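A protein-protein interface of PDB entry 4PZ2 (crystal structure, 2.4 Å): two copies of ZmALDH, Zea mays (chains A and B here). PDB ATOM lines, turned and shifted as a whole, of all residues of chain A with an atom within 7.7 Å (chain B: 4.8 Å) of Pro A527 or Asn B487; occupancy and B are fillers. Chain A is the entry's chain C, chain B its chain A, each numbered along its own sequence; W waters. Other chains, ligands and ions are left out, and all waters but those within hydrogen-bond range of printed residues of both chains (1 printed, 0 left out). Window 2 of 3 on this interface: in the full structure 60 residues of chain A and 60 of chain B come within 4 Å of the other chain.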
ATOM      1  N   GLY A 178     -20.186   5.617  -7.886  1.00  0.00           N
ATOM      2  CA  GLY A 178     -19.108   6.587  -7.723  1.00  0.00           C
ATOM      3  C   GLY A 178     -17.865   6.194  -8.498  1.00  0.00           C
ATOM      4  O   GLY A 178     -17.965   5.497  -9.517  1.00  0.00           O
ATOM      5  N   GLN A 179     -16.675   6.614  -8.009  1.00  0.00           N
ATOM      6  CA  GLN A 179     -15.382   6.308  -8.623  1.00  0.00           C
ATOM      7  C   GLN A 179     -14.980   4.849  -8.388  1.00  0.00           C
ATOM      8  O   GLN A 179     -14.062   4.540  -7.615  1.00  0.00           O
ATOM      9  CB  GLN A 179     -14.303   7.315  -8.180  1.00  0.00           C
ATOM     10  CG  GLN A 179     -14.394   8.667  -8.899  1.00  0.00           C
ATOM     11  CD  GLN A 179     -13.798   8.698 -10.299  1.00  0.00           C
ATOM     12  OE1 GLN A 179     -12.720   8.146 -10.586  1.00  0.00           O
ATOM     13  NE2 GLN A 179     -14.465   9.414 -11.195  1.00  0.00           N
ATOM     14  N   PHE A 180     -15.707   3.953  -9.065  1.00  0.00           N
ATOM     15  CA  PHE A 180     -15.565   2.489  -9.025  1.00  0.00           C
ATOM     16  C   PHE A 180     -15.771   1.911 -10.414  1.00  0.00           C
ATOM     17  O   PHE A 180     -16.536   2.474 -11.209  1.00  0.00           O
ATOM     18  CB  PHE A 180     -16.634   1.854  -8.103  1.00  0.00           C
ATOM     19  CG  PHE A 180     -16.481   2.199  -6.648  1.00  0.00           C
ATOM     20  CD1 PHE A 180     -15.581   1.502  -5.842  1.00  0.00           C
ATOM     21  CD2 PHE A 180     -17.219   3.230  -6.080  1.00  0.00           C
ATOM     22  CE1 PHE A 180     -15.407   1.849  -4.496  1.00  0.00           C
ATOM     23  CE2 PHE A 180     -17.053   3.570  -4.728  1.00  0.00           C
ATOM     24  CZ  PHE A 180     -16.145   2.882  -3.948  1.00  0.00           C
ATOM     25  N   GLN A 181     -15.127   0.768 -10.691  1.00  0.00           N
ATOM     26  CA  GLN A 181     -15.303   0.016 -11.927  1.00  0.00           C
ATOM     27  C   GLN A 181     -15.826  -1.339 -11.491  1.00  0.00           C
ATOM     28  O   GLN A 181     -15.214  -2.017 -10.661  1.00  0.00           O
ATOM     29  CB  GLN A 181     -13.986  -0.133 -12.692  1.00  0.00           C
ATOM     30  CG  GLN A 181     -14.143  -0.723 -14.095  1.00  0.00           C
ATOM     31  CD  GLN A 181     -12.840  -0.686 -14.864  1.00  0.00           C
ATOM     32  OE1 GLN A 181     -12.623   0.170 -15.744  1.00  0.00           O
ATOM     33  NE2 GLN A 181     -11.951  -1.630 -14.563  1.00  0.00           N
ATOM     34  N   GLY A 182     -16.995  -1.693 -11.990  1.00  0.00           N
ATOM     35  CA  GLY A 182     -17.638  -2.957 -11.675  1.00  0.00           C
ATOM     36  C   GLY A 182     -17.941  -3.762 -12.914  1.00  0.00           C
ATOM     37  O   GLY A 182     -18.324  -3.209 -13.945  1.00  0.00           O
ATOM     38  N   VAL A 525     -15.593  -5.608  -8.168  1.00  0.00           N
ATOM     39  CA  VAL A 525     -15.610  -4.168  -7.879  1.00  0.00           C
ATOM     40  C   VAL A 525     -14.237  -3.666  -7.434  1.00  0.00           C
ATOM     41  O   VAL A 525     -13.606  -4.245  -6.534  1.00  0.00           O
ATOM     42  CB  VAL A 525     -16.716  -3.787  -6.837  1.00  0.00           C
ATOM     43  CG1 VAL A 525     -16.702  -2.291  -6.506  1.00  0.00           C
ATOM     44  CG2 VAL A 525     -18.102  -4.221  -7.298  1.00  0.00           C
ATOM     45  N   THR A 526     -13.791  -2.553  -8.048  1.00  0.00           N
ATOM     46  CA  THR A 526     -12.548  -1.894  -7.690  1.00  0.00           C
ATOM     47  C   THR A 526     -12.706  -0.366  -7.725  1.00  0.00           C
ATOM     48  O   THR A 526     -13.429   0.124  -8.588  1.00  0.00           O
ATOM     49  CB  THR A 526     -11.344  -2.438  -8.513  1.00  0.00           C
ATOM     50  OG1 THR A 526     -10.139  -2.088  -7.833  1.00  0.00           O
ATOM     51  CG2 THR A 526     -11.290  -1.902  -9.954  1.00  0.00           C
ATOM     52  N   PRO A 527     -12.016   0.412  -6.844  1.00  0.00           N
ATOM     53  CA  PRO A 527     -12.083   1.876  -6.967  1.00  0.00           C
ATOM     54  C   PRO A 527     -11.336   2.361  -8.211  1.00  0.00           C
ATOM     55  O   PRO A 527     -10.488   1.657  -8.765  1.00  0.00           O
ATOM     56  CB  PRO A 527     -11.363   2.383  -5.702  1.00  0.00           C
ATOM     57  CG  PRO A 527     -11.147   1.205  -4.843  1.00  0.00           C
ATOM     58  CD  PRO A 527     -11.109   0.023  -5.742  1.00  0.00           C
ATOM     59  N   LEU A 528     -11.655   3.572  -8.641  1.00  0.00           N
ATOM     60  CA  LEU A 528     -10.989   4.213  -9.759  1.00  0.00           C
ATOM     61  C   LEU A 528     -10.350   5.461  -9.234  1.00  0.00           C
ATOM     62  O   LEU A 528     -10.922   6.119  -8.355  1.00  0.00           O
ATOM     63  CB  LEU A 528     -11.972   4.604 -10.877  1.00  0.00           C
ATOM     64  CG  LEU A 528     -12.640   3.482 -11.645  1.00  0.00           C
ATOM     65  CD1 LEU A 528     -13.795   4.035 -12.451  1.00  0.00           C
ATOM     66  CD2 LEU A 528     -11.626   2.740 -12.525  1.00  0.00           C
ATOM     67  N   ARG A 529      -9.167   5.785  -9.764  1.00  0.00           N
ATOM     68  CA  ARG A 529      -8.479   7.004  -9.416  1.00  0.00           C
ATOM     69  C   ARG A 529      -8.549   7.951 -10.603  1.00  0.00           C
ATOM     70  O   ARG A 529      -8.110   7.603 -11.701  1.00  0.00           O
ATOM     71  CB  ARG A 529      -7.040   6.724  -8.940  1.00  0.00           C
ATOM     72  CG  ARG A 529      -6.988   6.398  -7.430  1.00  0.00           C
ATOM     73  CD  ARG A 529      -7.179   4.940  -7.063  1.00  0.00           C
ATOM     74  NE  ARG A 529      -7.722   4.766  -5.707  1.00  0.00           N
ATOM     75  CZ  ARG A 529      -7.715   3.625  -5.016  1.00  0.00           C
ATOM     76  NH1 ARG A 529      -7.171   2.527  -5.534  1.00  0.00           N
ATOM     77  NH2 ARG A 529      -8.247   3.574  -3.805  1.00  0.00           N
ATOM     78  N   ALA A 530      -9.206   9.102 -10.389  1.00  0.00           N
ATOM     79  CA  ALA A 530      -9.372  10.210 -11.343  1.00  0.00           C
ATOM     80  C   ALA A 530      -9.885   9.835 -12.753  1.00  0.00           C
ATOM     81  O   ALA A 530      -9.336  10.278 -13.763  1.00  0.00           O
ATOM     82  CB  ALA A 530      -8.087  11.028 -11.415  1.00  0.00           C
ATOM     83  N   MET B 315      -3.884   1.607   4.801  1.00  0.00           N
ATOM     84  CA  MET B 315      -5.183   1.467   4.126  1.00  0.00           C
ATOM     85  C   MET B 315      -5.747   0.053   4.292  1.00  0.00           C
ATOM     86  O   MET B 315      -6.950  -0.089   4.480  1.00  0.00           O
ATOM     87  CB  MET B 315      -5.195   2.009   2.647  1.00  0.00           C
ATOM     88  CG  MET B 315      -4.787   1.007   1.521  1.00  0.00           C
ATOM     89  SD  MET B 315      -5.946  -0.340   1.038  1.00  0.00           S
ATOM     90  CE  MET B 315      -7.119   0.513   0.109  1.00  0.00           C
ATOM     91  N   LEU B 319      -9.159  -0.961   6.120  1.00  0.00           N
ATOM     92  CA  LEU B 319     -10.114  -1.693   5.297  1.00  0.00           C
ATOM     93  C   LEU B 319     -10.554  -2.971   6.004  1.00  0.00           C
ATOM     94  O   LEU B 319     -11.756  -3.265   6.026  1.00  0.00           O
ATOM     95  CB  LEU B 319      -9.500  -2.009   3.921  1.00  0.00           C
ATOM     96  CG  LEU B 319     -10.445  -2.477   2.812  1.00  0.00           C
ATOM     97  CD1 LEU B 319     -11.339  -1.347   2.337  1.00  0.00           C
ATOM     98  CD2 LEU B 319      -9.658  -3.009   1.642  1.00  0.00           C
ATOM     99  N   VAL B 464      -9.496  -8.650  -2.173  1.00  0.00           N
ATOM    100  CA  VAL B 464      -8.075  -8.694  -2.557  1.00  0.00           C
ATOM    101  C   VAL B 464      -7.496  -7.306  -2.399  1.00  0.00           C
ATOM    102  O   VAL B 464      -8.022  -6.348  -2.969  1.00  0.00           O
ATOM    103  CB  VAL B 464      -7.729  -9.184  -3.998  1.00  0.00           C
ATOM    104  CG1 VAL B 464      -6.401  -9.934  -4.010  1.00  0.00           C
ATOM    105  CG2 VAL B 464      -8.835  -9.999  -4.642  1.00  0.00           C
ATOM    106  N   VAL B 465      -6.378  -7.202  -1.690  1.00  0.00           N
ATOM    107  CA  VAL B 465      -5.673  -5.930  -1.567  1.00  0.00           C
ATOM    108  C   VAL B 465      -4.289  -6.104  -2.202  1.00  0.00           C
ATOM    109  O   VAL B 465      -3.451  -6.830  -1.666  1.00  0.00           O
ATOM    110  CB  VAL B 465      -5.637  -5.339  -0.131  1.00  0.00           C
ATOM    111  CG1 VAL B 465      -5.113  -3.901  -0.156  1.00  0.00           C
ATOM    112  CG2 VAL B 465      -7.018  -5.387   0.513  1.00  0.00           C
ATOM    113  N   THR B 466      -4.109  -5.503  -3.397  1.00  0.00           N
ATOM    114  CA  THR B 466      -2.886  -5.527  -4.211  1.00  0.00           C
ATOM    115  C   THR B 466      -2.867  -4.385  -5.243  1.00  0.00           C
ATOM    116  O   THR B 466      -3.920  -3.954  -5.714  1.00  0.00           O
ATOM    117  CB  THR B 466      -2.694  -6.919  -4.889  1.00  0.00           C
ATOM    118  OG1 THR B 466      -1.424  -6.974  -5.520  1.00  0.00           O
ATOM    119  CG2 THR B 466      -3.776  -7.263  -5.910  1.00  0.00           C
ATOM    120  N   TRP B 485     -14.201  -7.999  -4.079  1.00  0.00           N
ATOM    121  CA  TRP B 485     -13.807  -6.597  -3.962  1.00  0.00           C
ATOM    122  C   TRP B 485     -12.289  -6.499  -4.100  1.00  0.00           C
ATOM    123  O   TRP B 485     -11.571  -7.300  -3.514  1.00  0.00           O
ATOM    124  CB  TRP B 485     -14.265  -6.016  -2.609  1.00  0.00           C
ATOM    125  CG  TRP B 485     -15.740  -5.765  -2.533  1.00  0.00           C
ATOM    126  CD1 TRP B 485     -16.433  -4.771  -3.159  1.00  0.00           C
ATOM    127  CD2 TRP B 485     -16.712  -6.566  -1.857  1.00  0.00           C
ATOM    128  NE1 TRP B 485     -17.775  -4.912  -2.929  1.00  0.00           N
ATOM    129  CE2 TRP B 485     -17.977  -5.997  -2.117  1.00  0.00           C
ATOM    130  CE3 TRP B 485     -16.641  -7.722  -1.064  1.00  0.00           C
ATOM    131  CZ2 TRP B 485     -19.158  -6.523  -1.587  1.00  0.00           C
ATOM    132  CZ3 TRP B 485     -17.807  -8.230  -0.525  1.00  0.00           C
ATOM    133  CH2 TRP B 485     -19.046  -7.619  -0.769  1.00  0.00           C
ATOM    134  N   VAL B 486     -11.805  -5.566  -4.926  1.00  0.00           N
ATOM    135  CA  VAL B 486     -10.377  -5.344  -5.141  1.00  0.00           C
ATOM    136  C   VAL B 486     -10.080  -3.962  -4.619  1.00  0.00           C
ATOM    137  O   VAL B 486     -10.652  -3.017  -5.119  1.00  0.00           O
ATOM    138  CB  VAL B 486      -9.962  -5.491  -6.637  1.00  0.00           C
ATOM    139  CG1 VAL B 486      -8.447  -5.368  -6.806  1.00  0.00           C
ATOM    140  CG2 VAL B 486     -10.476  -6.800  -7.234  1.00  0.00           C
ATOM    141  N   ASN B 487      -9.225  -3.842  -3.610  1.00  0.00           N
ATOM    142  CA  ASN B 487      -8.786  -2.565  -3.002  1.00  0.00           C
ATOM    143  C   ASN B 487      -9.898  -1.708  -2.386  1.00  0.00           C
ATOM    144  O   ASN B 487      -9.784  -0.477  -2.273  1.00  0.00           O
ATOM    145  CB  ASN B 487      -7.884  -1.757  -3.954  1.00  0.00           C
ATOM    146  CG  ASN B 487      -6.661  -2.522  -4.393  1.00  0.00           C
ATOM    147  OD1 ASN B 487      -6.046  -3.266  -3.612  1.00  0.00           O
ATOM    148  ND2 ASN B 487      -6.281  -2.355  -5.655  1.00  0.00           N
ATOM    149  N   CYS B 488     -10.960  -2.396  -1.955  1.00  0.00           N
ATOM    150  CA  CYS B 488     -12.161  -1.855  -1.339  1.00  0.00           C
ATOM    151  C   CYS B 488     -12.933  -3.027  -0.735  1.00  0.00           C
ATOM    152  O   CYS B 488     -12.465  -4.166  -0.801  1.00  0.00           O
ATOM    153  CB  CYS B 488     -13.007  -1.084  -2.363  1.00  0.00           C
ATOM    154  SG  CYS B 488     -13.715  -2.101  -3.696  1.00  0.00           S
HETATM  155  O   HOH W   1      -7.758  -0.555  -7.238  1.00  0.00           O
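Printed residues of chain A that touch a printed residue of chain B: Val A525, Thr A526 and Pro A527. Hydrophobic or aromatic side chains of chain B that line the printed part of chain A: Trp B485 and Val B486. Among the printed residues, 7 pairs touch across the chains.
The backbone NH (N) of Val B464 sits at hydrogen-bond distance from the backbone carbonyl oxygen (O) of Trp B485. The backbone carbonyl oxygen (O) of Val B464 lies within hydrogen-bond range of the backbone NH (N) of Asn B487 (2.9 Å). The backbone carbonyl oxygen (O) of Thr B466 sits at hydrogen-bond distance from the side-chain amide nitrogen (ND2) of Asn B487, 2.9 Å away. SG of Cys B488 lies within hydrogen-bond range of O of Val B486, 3.5 Å away. The backbone NH (N) of Gln A181 is in hydrogen-bond range of the backbone carbonyl oxygen (O) of Thr A526, 2.8 Å away.
Printed residues of chain B within 4 Å of Pro A527: Val B486, Asn B487 and Cys B488. Asn B487 touches one residue of chain A. Of the printed residues of chain B, Thr A526 touches Val B486. Of the printed residues of chain A, Cys B488 touches Val A525 and Pro A527. Printed residues of chain A within 4 Å of Val B486: Val A525 (2.8 Å), Thr A526 (2.9 Å) and Pro A527 (3.1 Å). Of the printed residues of chain B, Val A525 touches Trp B485, Val B486 and Cys B488. The nearest printed residue of chain B that does not touch Thr A526 is Cys B488 (4.2 Å).
Water W1 bridges the side-chain amide nitrogen of Asn B487 (2.8 Å) and the side-chain hydroxyl of Thr A526 (2.9 Å).
The backbone NH (N) of Val B486 is in hydrogen-bond range of the backbone carbonyl oxygen (O) of Val A525 (2.8 Å). The backbone carbonyl oxygen (O) of Val B486 sits at hydrogen-bond distance from the side-chain hydroxyl (OG1) of Thr A526 (2.9 Å). The backbone carbonyl oxygen (O) of Val A525 is in hydrogen-bond range of the side-chain sulfur (SG) of Cys B488 (3.6 Å).
No position is printed for both chains.
Among the printed residues, merely in contact across the chains: Val A525 with Trp B485, Pro A527 with Val B486, Pro A527 with Asn B487 and Pro A527 with Cys B488.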
